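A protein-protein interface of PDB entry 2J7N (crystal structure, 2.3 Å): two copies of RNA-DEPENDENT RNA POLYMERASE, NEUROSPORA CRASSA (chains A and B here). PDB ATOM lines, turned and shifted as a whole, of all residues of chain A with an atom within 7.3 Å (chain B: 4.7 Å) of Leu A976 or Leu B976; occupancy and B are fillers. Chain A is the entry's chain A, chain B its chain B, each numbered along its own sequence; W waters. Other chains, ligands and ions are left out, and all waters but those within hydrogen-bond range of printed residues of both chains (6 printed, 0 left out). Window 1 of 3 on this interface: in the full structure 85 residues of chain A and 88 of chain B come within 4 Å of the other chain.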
ATOM      1  N   ARG A 462      27.276  23.730  24.336  1.00  0.00           N
ATOM      2  CA  ARG A 462      27.222  22.987  23.080  1.00  0.00           C
ATOM      3  C   ARG A 462      26.191  23.564  22.092  1.00  0.00           C
ATOM      4  O   ARG A 462      26.484  23.738  20.913  1.00  0.00           O
ATOM      5  CB  ARG A 462      26.961  21.501  23.334  1.00  0.00           C
ATOM      6  CG  ARG A 462      26.911  20.675  22.060  1.00  0.00           C
ATOM      7  CD  ARG A 462      26.653  19.206  22.349  1.00  0.00           C
ATOM      8  NE  ARG A 462      25.357  19.001  22.998  1.00  0.00           N
ATOM      9  CZ  ARG A 462      24.890  17.819  23.388  1.00  0.00           C
ATOM     10  NH1 ARG A 462      25.632  16.724  23.177  1.00  0.00           N
ATOM     11  NH2 ARG A 462      23.687  17.733  23.983  1.00  0.00           N
ATOM     12  N   TYR A 466      27.220  25.368  18.645  1.00  0.00           N
ATOM     13  CA  TYR A 466      26.654  24.871  17.398  1.00  0.00           C
ATOM     14  C   TYR A 466      25.959  25.982  16.597  1.00  0.00           C
ATOM     15  O   TYR A 466      26.096  26.066  15.376  1.00  0.00           O
ATOM     16  CB  TYR A 466      25.696  23.701  17.682  1.00  0.00           C
ATOM     17  CG  TYR A 466      24.927  23.254  16.474  1.00  0.00           C
ATOM     18  CD1 TYR A 466      25.479  22.364  15.564  1.00  0.00           C
ATOM     19  CD2 TYR A 466      23.649  23.746  16.225  1.00  0.00           C
ATOM     20  CE1 TYR A 466      24.772  21.976  14.432  1.00  0.00           C
ATOM     21  CE2 TYR A 466      22.932  23.359  15.106  1.00  0.00           C
ATOM     22  CZ  TYR A 466      23.499  22.482  14.215  1.00  0.00           C
ATOM     23  OH  TYR A 466      22.781  22.103  13.114  1.00  0.00           O
ATOM     24  N   ARG A 475      31.446  19.107   7.109  1.00  0.00           N
ATOM     25  CA  ARG A 475      31.074  17.737   7.457  1.00  0.00           C
ATOM     26  C   ARG A 475      30.562  16.920   6.247  1.00  0.00           C
ATOM     27  O   ARG A 475      30.949  15.759   6.070  1.00  0.00           O
ATOM     28  CB  ARG A 475      30.036  17.745   8.577  1.00  0.00           C
ATOM     29  CG  ARG A 475      30.521  18.385   9.881  1.00  0.00           C
ATOM     30  CD  ARG A 475      29.410  18.380  10.937  1.00  0.00           C
ATOM     31  NE  ARG A 475      29.948  18.370  12.295  1.00  0.00           N
ATOM     32  CZ  ARG A 475      29.364  17.781  13.344  1.00  0.00           C
ATOM     33  NH1 ARG A 475      28.206  17.137  13.204  1.00  0.00           N
ATOM     34  NH2 ARG A 475      29.945  17.831  14.543  1.00  0.00           N
ATOM     35  N   GLU A 493      34.283  23.046  16.749  1.00  0.00           N
ATOM     36  CA  GLU A 493      34.137  21.603  16.660  1.00  0.00           C
ATOM     37  C   GLU A 493      34.939  20.941  17.769  1.00  0.00           C
ATOM     38  O   GLU A 493      34.524  19.934  18.327  1.00  0.00           O
ATOM     39  CB  GLU A 493      34.632  21.152  15.283  1.00  0.00           C
ATOM     40  CG  GLU A 493      34.025  19.896  14.746  1.00  0.00           C
ATOM     41  CD  GLU A 493      32.540  20.007  14.409  1.00  0.00           C
ATOM     42  OE1 GLU A 493      32.185  20.536  13.333  1.00  0.00           O
ATOM     43  OE2 GLU A 493      31.731  19.497  15.213  1.00  0.00           O
ATOM     44  N   ASN A 500      31.266  16.586  24.480  1.00  0.00           N
ATOM     45  CA  ASN A 500      30.505  15.363  24.209  1.00  0.00           C
ATOM     46  C   ASN A 500      31.108  14.124  24.900  1.00  0.00           C
ATOM     47  O   ASN A 500      30.420  13.120  25.099  1.00  0.00           O
ATOM     48  CB  ASN A 500      30.379  15.132  22.702  1.00  0.00           C
ATOM     49  CG  ASN A 500      29.300  16.000  22.069  1.00  0.00           C
ATOM     50  OD1 ASN A 500      28.288  16.327  22.699  1.00  0.00           O
ATOM     51  ND2 ASN A 500      29.499  16.356  20.810  1.00  0.00           N
ATOM     52  N   MET A 968      30.786   6.243  18.786  1.00  0.00           N
ATOM     53  CA  MET A 968      30.276   6.578  17.468  1.00  0.00           C
ATOM     54  C   MET A 968      31.382   6.577  16.436  1.00  0.00           C
ATOM     55  O   MET A 968      32.499   6.946  16.733  1.00  0.00           O
ATOM     56  CB  MET A 968      29.599   7.927  17.568  1.00  0.00           C
ATOM     57  CG  MET A 968      28.436   7.843  18.530  1.00  0.00           C
ATOM     58  SD  MET A 968      27.152   9.006  18.097  1.00  0.00           S
ATOM     59  CE  MET A 968      26.995   8.730  16.335  1.00  0.00           C
ATOM     60  N   PHE A 971      32.011   8.969  10.828  1.00  0.00           N
ATOM     61  CA  PHE A 971      30.938   9.298   9.907  1.00  0.00           C
ATOM     62  C   PHE A 971      29.609   9.552  10.599  1.00  0.00           C
ATOM     63  O   PHE A 971      28.947  10.555  10.331  1.00  0.00           O
ATOM     64  CB  PHE A 971      30.718   8.190   8.891  1.00  0.00           C
ATOM     65  CG  PHE A 971      29.496   8.418   8.052  1.00  0.00           C
ATOM     66  CD1 PHE A 971      29.446   9.490   7.167  1.00  0.00           C
ATOM     67  CD2 PHE A 971      28.390   7.610   8.174  1.00  0.00           C
ATOM     68  CE1 PHE A 971      28.322   9.739   6.422  1.00  0.00           C
ATOM     69  CE2 PHE A 971      27.264   7.861   7.414  1.00  0.00           C
ATOM     70  CZ  PHE A 971      27.233   8.918   6.538  1.00  0.00           C
ATOM     71  N   MET A 972      29.204   8.618  11.466  1.00  0.00           N
ATOM     72  CA  MET A 972      27.906   8.710  12.133  1.00  0.00           C
ATOM     73  C   MET A 972      27.848   9.875  13.120  1.00  0.00           C
ATOM     74  O   MET A 972      26.789  10.506  13.308  1.00  0.00           O
ATOM     75  CB  MET A 972      27.499   7.372  12.765  1.00  0.00           C
ATOM     76  CG  MET A 972      27.178   6.295  11.703  1.00  0.00           C
ATOM     77  SD  MET A 972      25.828   6.734  10.572  1.00  0.00           S
ATOM     78  CE  MET A 972      24.478   5.839  11.361  1.00  0.00           C
ATOM     79  N   TYR A 973      28.990  10.208  13.701  1.00  0.00           N
ATOM     80  CA  TYR A 973      29.062  11.374  14.574  1.00  0.00           C
ATOM     81  C   TYR A 973      28.840  12.673  13.788  1.00  0.00           C
ATOM     82  O   TYR A 973      28.160  13.572  14.269  1.00  0.00           O
ATOM     83  CB  TYR A 973      30.395  11.379  15.345  1.00  0.00           C
ATOM     84  CG  TYR A 973      30.691  12.609  16.185  1.00  0.00           C
ATOM     85  CD1 TYR A 973      30.359  12.652  17.530  1.00  0.00           C
ATOM     86  CD2 TYR A 973      31.341  13.720  15.634  1.00  0.00           C
ATOM     87  CE1 TYR A 973      30.641  13.774  18.315  1.00  0.00           C
ATOM     88  CE2 TYR A 973      31.635  14.850  16.407  1.00  0.00           C
ATOM     89  CZ  TYR A 973      31.285  14.868  17.759  1.00  0.00           C
ATOM     90  OH  TYR A 973      31.579  15.987  18.545  1.00  0.00           O
ATOM     91  N   ALA A 974      29.392  12.765  12.582  1.00  0.00           N
ATOM     92  CA  ALA A 974      29.238  13.984  11.767  1.00  0.00           C
ATOM     93  C   ALA A 974      27.795  14.292  11.368  1.00  0.00           C
ATOM     94  O   ALA A 974      27.492  15.421  11.011  1.00  0.00           O
ATOM     95  CB  ALA A 974      30.114  13.938  10.541  1.00  0.00           C
ATOM     96  N   GLY A 975      26.914  13.297  11.442  1.00  0.00           N
ATOM     97  CA  GLY A 975      25.535  13.447  10.969  1.00  0.00           C
ATOM     98  C   GLY A 975      24.516  13.915  11.997  1.00  0.00           C
ATOM     99  O   GLY A 975      23.376  14.194  11.662  1.00  0.00           O
ATOM    100  N   LEU A 976      24.939  14.001  13.250  1.00  0.00           N
ATOM    101  CA  LEU A 976      24.084  14.438  14.352  1.00  0.00           C
ATOM    102  C   LEU A 976      24.323  15.883  14.677  1.00  0.00           C
ATOM    103  O   LEU A 976      25.456  16.368  14.565  1.00  0.00           O
ATOM    104  CB  LEU A 976      24.411  13.674  15.640  1.00  0.00           C
ATOM    105  CG  LEU A 976      24.401  12.167  15.546  1.00  0.00           C
ATOM    106  CD1 LEU A 976      24.936  11.557  16.852  1.00  0.00           C
ATOM    107  CD2 LEU A 976      23.001  11.703  15.230  1.00  0.00           C
ATOM    108  N   MET A 977      23.270  16.540  15.158  1.00  0.00           N
ATOM    109  CA  MET A 977      23.328  17.922  15.614  1.00  0.00           C
ATOM    110  C   MET A 977      22.695  18.023  17.008  1.00  0.00           C
ATOM    111  O   MET A 977      21.896  17.166  17.399  1.00  0.00           O
ATOM    112  CB  MET A 977      22.556  18.833  14.633  1.00  0.00           C
ATOM    113  CG  MET A 977      21.090  18.424  14.462  1.00  0.00           C
ATOM    114  SD  MET A 977      20.190  19.409  13.237  1.00  0.00           S
ATOM    115  CE  MET A 977      19.852  20.926  14.138  1.00  0.00           C
ATOM    116  N   PRO A 978      23.051  19.066  17.773  1.00  0.00           N
ATOM    117  CA  PRO A 978      22.357  19.257  19.038  1.00  0.00           C
ATOM    118  C   PRO A 978      20.853  19.471  18.827  1.00  0.00           C
ATOM    119  O   PRO A 978      20.429  20.163  17.895  1.00  0.00           O
ATOM    120  CB  PRO A 978      23.026  20.513  19.623  1.00  0.00           C
ATOM    121  CG  PRO A 978      24.367  20.573  18.976  1.00  0.00           C
ATOM    122  CD  PRO A 978      24.110  20.074  17.573  1.00  0.00           C
ATOM    123  N   ASP A 979      20.064  18.848  19.689  1.00  0.00           N
ATOM    124  CA  ASP A 979      18.612  18.931  19.649  1.00  0.00           C
ATOM    125  C   ASP A 979      18.173  20.077  20.564  1.00  0.00           C
ATOM    126  O   ASP A 979      18.150  19.940  21.785  1.00  0.00           O
ATOM    127  CB  ASP A 979      18.042  17.613  20.156  1.00  0.00           C
ATOM    128  CG  ASP A 979      16.544  17.595  20.191  1.00  0.00           C
ATOM    129  OD1 ASP A 979      15.912  18.620  19.895  1.00  0.00           O
ATOM    130  OD2 ASP A 979      15.989  16.540  20.532  1.00  0.00           O
ATOM    131  N   PHE A 982      15.511  19.280  23.112  1.00  0.00           N
ATOM    132  CA  PHE A 982      16.060  18.533  24.241  1.00  0.00           C
ATOM    133  C   PHE A 982      16.675  19.495  25.249  1.00  0.00           C
ATOM    134  O   PHE A 982      16.251  19.569  26.409  1.00  0.00           O
ATOM    135  CB  PHE A 982      17.103  17.482  23.795  1.00  0.00           C
ATOM    136  CG  PHE A 982      17.792  16.807  24.946  1.00  0.00           C
ATOM    137  CD1 PHE A 982      17.236  15.684  25.545  1.00  0.00           C
ATOM    138  CD2 PHE A 982      18.965  17.324  25.475  1.00  0.00           C
ATOM    139  CE1 PHE A 982      17.869  15.077  26.636  1.00  0.00           C
ATOM    140  CE2 PHE A 982      19.590  16.720  26.580  1.00  0.00           C
ATOM    141  CZ  PHE A 982      19.046  15.607  27.146  1.00  0.00           C
ATOM    142  N   ARG B 462      18.738   5.654   9.806  1.00  0.00           N
ATOM    143  CA  ARG B 462      18.781   6.360  11.071  1.00  0.00           C
ATOM    144  C   ARG B 462      17.810   7.559  11.063  1.00  0.00           C
ATOM    145  O   ARG B 462      17.110   7.784  12.047  1.00  0.00           O
ATOM    146  CB  ARG B 462      20.203   6.795  11.388  1.00  0.00           C
ATOM    147  CG  ARG B 462      20.336   7.609  12.663  1.00  0.00           C
ATOM    148  CD  ARG B 462      21.114   8.870  12.356  1.00  0.00           C
ATOM    149  NE  ARG B 462      22.456   8.826  12.898  1.00  0.00           N
ATOM    150  CZ  ARG B 462      23.492   9.489  12.389  1.00  0.00           C
ATOM    151  NH1 ARG B 462      23.368  10.244  11.287  1.00  0.00           N
ATOM    152  NH2 ARG B 462      24.660   9.387  12.988  1.00  0.00           N
ATOM    153  N   ARG B 475      14.064  10.710  26.864  1.00  0.00           N
ATOM    154  CA  ARG B 475      15.456  11.158  27.005  1.00  0.00           C
ATOM    155  C   ARG B 475      15.541  12.310  27.993  1.00  0.00           C
ATOM    156  O   ARG B 475      16.448  12.359  28.816  1.00  0.00           O
ATOM    157  CB  ARG B 475      16.045  11.594  25.656  1.00  0.00           C
ATOM    158  CG  ARG B 475      16.590  10.466  24.802  1.00  0.00           C
ATOM    159  CD  ARG B 475      16.741  10.958  23.373  1.00  0.00           C
ATOM    160  NE  ARG B 475      17.193   9.939  22.437  1.00  0.00           N
ATOM    161  CZ  ARG B 475      18.227  10.083  21.606  1.00  0.00           C
ATOM    162  NH1 ARG B 475      18.935  11.220  21.585  1.00  0.00           N
ATOM    163  NH2 ARG B 475      18.549   9.102  20.775  1.00  0.00           N
ATOM    164  N   MET B 968      31.044   9.292  23.312  1.00  0.00           N
ATOM    165  CA  MET B 968      30.102  10.172  23.960  1.00  0.00           C
ATOM    166  C   MET B 968      29.546   9.642  25.285  1.00  0.00           C
ATOM    167  O   MET B 968      29.343   8.438  25.455  1.00  0.00           O
ATOM    168  CB  MET B 968      28.999  10.489  22.965  1.00  0.00           C
ATOM    169  CG  MET B 968      29.612  11.084  21.732  1.00  0.00           C
ATOM    170  SD  MET B 968      28.460  12.007  20.772  1.00  0.00           S
ATOM    171  CE  MET B 968      27.554  12.972  21.971  1.00  0.00           C
ATOM    172  N   MET B 972      25.342  13.181  27.042  1.00  0.00           N
ATOM    173  CA  MET B 972      25.641  14.005  25.865  1.00  0.00           C
ATOM    174  C   MET B 972      25.143  13.367  24.555  1.00  0.00           C
ATOM    175  O   MET B 972      24.698  14.073  23.633  1.00  0.00           O
ATOM    176  CB  MET B 972      27.127  14.415  25.826  1.00  0.00           C
ATOM    177  CG  MET B 972      27.513  15.424  26.920  1.00  0.00           C
ATOM    178  SD  MET B 972      26.588  17.000  26.868  1.00  0.00           S
ATOM    179  CE  MET B 972      27.690  18.019  25.856  1.00  0.00           C
ATOM    180  N   TYR B 973      25.173  12.043  24.486  1.00  0.00           N
ATOM    181  CA  TYR B 973      24.508  11.327  23.375  1.00  0.00           C
ATOM    182  C   TYR B 973      22.989  11.586  23.314  1.00  0.00           C
ATOM    183  O   TYR B 973      22.426  11.799  22.233  1.00  0.00           O
ATOM    184  CB  TYR B 973      24.740   9.842  23.518  1.00  0.00           C
ATOM    185  CG  TYR B 973      24.080   8.958  22.494  1.00  0.00           C
ATOM    186  CD1 TYR B 973      22.901   8.275  22.783  1.00  0.00           C
ATOM    187  CD2 TYR B 973      24.671   8.734  21.264  1.00  0.00           C
ATOM    188  CE1 TYR B 973      22.321   7.416  21.857  1.00  0.00           C
ATOM    189  CE2 TYR B 973      24.106   7.881  20.345  1.00  0.00           C
ATOM    190  CZ  TYR B 973      22.927   7.226  20.633  1.00  0.00           C
ATOM    191  OH  TYR B 973      22.368   6.380  19.679  1.00  0.00           O
ATOM    192  N   ALA B 974      22.333  11.557  24.473  1.00  0.00           N
ATOM    193  CA  ALA B 974      20.887  11.734  24.543  1.00  0.00           C
ATOM    194  C   ALA B 974      20.431  13.057  23.929  1.00  0.00           C
ATOM    195  O   ALA B 974      19.297  13.172  23.470  1.00  0.00           O
ATOM    196  CB  ALA B 974      20.432  11.652  25.980  1.00  0.00           C
ATOM    197  N   GLY B 975      21.303  14.062  23.926  1.00  0.00           N
ATOM    198  CA  GLY B 975      20.905  15.417  23.499  1.00  0.00           C
ATOM    199  C   GLY B 975      21.113  15.769  22.044  1.00  0.00           C
ATOM    200  O   GLY B 975      20.836  16.888  21.627  1.00  0.00           O
ATOM    201  N   LEU B 976      21.632  14.814  21.284  1.00  0.00           N
ATOM    202  CA  LEU B 976      21.859  14.939  19.852  1.00  0.00           C
ATOM    203  C   LEU B 976      20.774  14.241  19.056  1.00  0.00           C
ATOM    204  O   LEU B 976      20.342  13.150  19.430  1.00  0.00           O
ATOM    205  CB  LEU B 976      23.195  14.269  19.509  1.00  0.00           C
ATOM    206  CG  LEU B 976      24.433  14.927  20.104  1.00  0.00           C
ATOM    207  CD1 LEU B 976      25.608  14.191  19.585  1.00  0.00           C
ATOM    208  CD2 LEU B 976      24.505  16.416  19.705  1.00  0.00           C
ATOM    209  N   MET B 977      20.373  14.844  17.941  1.00  0.00           N
ATOM    210  CA  MET B 977      19.433  14.228  17.006  1.00  0.00           C
ATOM    211  C   MET B 977      20.082  14.064  15.615  1.00  0.00           C
ATOM    212  O   MET B 977      21.104  14.681  15.328  1.00  0.00           O
ATOM    213  CB  MET B 977      18.168  15.090  16.910  1.00  0.00           C
ATOM    214  CG  MET B 977      18.449  16.527  16.512  1.00  0.00           C
ATOM    215  SD  MET B 977      17.007  17.623  16.473  1.00  0.00           S
ATOM    216  CE  MET B 977      16.106  16.924  15.076  1.00  0.00           C
ATOM    217  N   PRO B 978      19.508  13.212  14.751  1.00  0.00           N
ATOM    218  CA  PRO B 978      19.998  13.204  13.373  1.00  0.00           C
ATOM    219  C   PRO B 978      19.736  14.561  12.701  1.00  0.00           C
ATOM    220  O   PRO B 978      18.686  15.179  12.916  1.00  0.00           O
ATOM    221  CB  PRO B 978      19.155  12.118  12.689  1.00  0.00           C
ATOM    222  CG  PRO B 978      18.543  11.322  13.771  1.00  0.00           C
ATOM    223  CD  PRO B 978      18.430  12.237  14.973  1.00  0.00           C
ATOM    224  N   ASP B 979      20.708  15.009  11.913  1.00  0.00           N
ATOM    225  CA  ASP B 979      20.659  16.272  11.204  1.00  0.00           C
ATOM    226  C   ASP B 979      20.124  15.969   9.795  1.00  0.00           C
ATOM    227  O   ASP B 979      20.834  15.378   8.981  1.00  0.00           O
ATOM    228  CB  ASP B 979      22.081  16.847  11.188  1.00  0.00           C
ATOM    229  CG  ASP B 979      22.226  18.086  10.336  1.00  0.00           C
ATOM    230  OD1 ASP B 979      21.236  18.564   9.725  1.00  0.00           O
ATOM    231  OD2 ASP B 979      23.365  18.592  10.288  1.00  0.00           O
HETATM  232  O   HOH W   1      18.920  19.906  10.040  1.00  0.00           O
HETATM  233  O   HOH W   2      21.308  19.134  23.413  1.00  0.00           O
HETATM  234  O   HOH W   3      22.029  12.387   9.686  1.00  0.00           O
HETATM  235  O   HOH W   4      17.020  14.511  22.051  1.00  0.00           O
HETATM  236  O   HOH W   5      26.137  17.854  10.615  1.00  0.00           O
HETATM  237  O   HOH W   6      22.953  16.240  26.095  1.00  0.00           O
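Of chain B, only Arg B462, Leu B976, Met B977 and Pro B978 come within 4 Å of Leu A976.
Of chain A, only Arg A462, Pro A978, Asp A979 and Phe A982 come within 4 Å of Gly B975.
Printed residues of chain B within 4 Å of Gly A975: Arg B462, Pro B978 and Asp B979.
Of the printed residues of chain A, Pro B978 touches Gly A975 (3.8 Å) and Leu A976 (3.8 Å).
Of the printed residues of chain A, Met B968 touches Asn A500 (3.2 Å) and Tyr A973 (3.7 Å).
Of the printed residues of chain A, Arg B475 touches Phe A982.
Of the printed residues of chain B, Arg A462 touches Met B972, Gly B975 and Leu B976.
Tyr A466 touches none of the printed residues of chain B.
Arg A475 touches none of the printed residues of chain B.
The nearest residue of chain B that does not touch Leu A976 is Asp B979 (4.2 Å).
The nearest residue of chain A that does not touch Leu B976 is Asp A979 (4.3 Å).
Arg A462 touches Leu B976, and with the chains exchanged Leu A976 touches Arg B462.
Gly A975 touches Asp B979, and with the chains exchanged Asp A979 touches Gly B975.
Leu A976 touches its own counterpart, Leu B976.
Met A977 touches Asp B979, and with the chains exchanged Asp A979 touches Met B977.
Water W6 lies within hydrogen-bond range of the guanidinium group of Arg A462, the backbone NH of Gly B975 and the side-chain sulfur of Met B972.
Water W1 lies within hydrogen-bond range of the side-chain carboxylate of Asp B979 (2.7 Å) and the side-chain sulfur of Met A977 (3.5 Å).
Water W4 bridges the side-chain carboxylate (OD2) of Asp A979 (2.7 Å) and the backbone carbonyl oxygen (O) of Ala B974 (3.0 Å).
Water W5 lies within hydrogen-bond range of O of Ala A974, OD2 of Asp B979 and NH1 of Arg A475.
Water W2 lies within hydrogen-bond range of the guanidinium group of Arg A462 (2.8 Å) and the backbone carbonyl oxygen of Gly B975 (2.9 Å).
Water W3 lies within hydrogen-bond range of NH1 of Arg B462 (3.0 Å), O of Gly A975 (3.0 Å) and O of Asp B979 (3.3 Å).
The backbone carbonyl oxygen (O) of Leu A976 is in hydrogen-bond range of the guanidinium group (NH1) of Arg A475 (3.2 Å).
OH of Tyr A973 is in hydrogen-bond range of ND2 of Asn A500 (3.1 Å).
The side-chain amide oxygen (OD1) of Asn A500 is in hydrogen-bond range of the guanidinium group (NH1) of Arg A462 (2.7 Å).
The guanidinium group of Arg B475 sits at hydrogen-bond distance from the backbone carbonyl oxygen of Ala B974, at 2.7 Å.
The side-chain sulfur of Met A977 sits close to the side-chain hydroxyl of Tyr A466.
The guanidinium group (NH1) of Arg B475 lies within hydrogen-bond range of the backbone carbonyl oxygen (O) of Leu B976, 3.2 Å away.
The backbone NH (N) of Asp A979 lies within hydrogen-bond range of the backbone carbonyl oxygen (O) of Gly B975 (2.9 Å).
OD1 of Asp A979 lies close to SD of Met B977 (3.7 Å).
The backbone NH (N) of Met B977 is in hydrogen-bond range of the backbone carbonyl oxygen (O) of Met A977 (2.8 Å).
NH1 of Arg A462 is in hydrogen-bond range of O of Met B972 (2.8 Å).
N of Asp B979 is in hydrogen-bond range of O of Gly A975 (2.8 Å).
The backbone carbonyl oxygen (O) of Met A972 lies within hydrogen-bond range of the guanidinium group (NH2) of Arg B462 (2.4 Å).
The side-chain sulfur (SD) of Met A977 sits close to the side-chain carboxylate (OD1) of Asp B979 (3.8 Å).
Along chain B the printed residues that touch a printed residue of chain A span positions 462 to 979.
Among the printed residues, 25 pairs touch across the chains.
Among the printed residues, no Asp or Glu carboxylate lies within 4 Å of a Lys or Arg side-chain nitrogen of the other chain.
Among the printed residues, merely in contact across the chains: Arg A462 with Gly B975 (3.7 Å), Arg A462 with Leu B976 (3.7 Å), Asn A500 with Met B968 (3.2 Å), Asn A500 with Met B972 (3.6 Å), Met A968 with Tyr B973 (3.9 Å), Tyr A973 with Met B968 (3.7 Å), Gly A975 with Arg B462 (3.9 Å), Gly A975 with Pro B978 (3.8 Å), Leu A976 with Arg B462 (3.6 Å), Leu A976 with Leu B976 (3.9 Å), Leu A976 with Met B977 (3.1 Å), Leu A976 with Pro B978 (3.8 Å), Met A977 with Leu B976 (3.3 Å), Pro A978 with Gly B975 (3.8 Å), Pro A978 with Leu B976 (3.6 Å), Phe A982 with Arg B475 (3.8 Å), Phe A982 with Ala B974 (3.9 Å) and Phe A982 with Gly B975 (3.4 Å).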
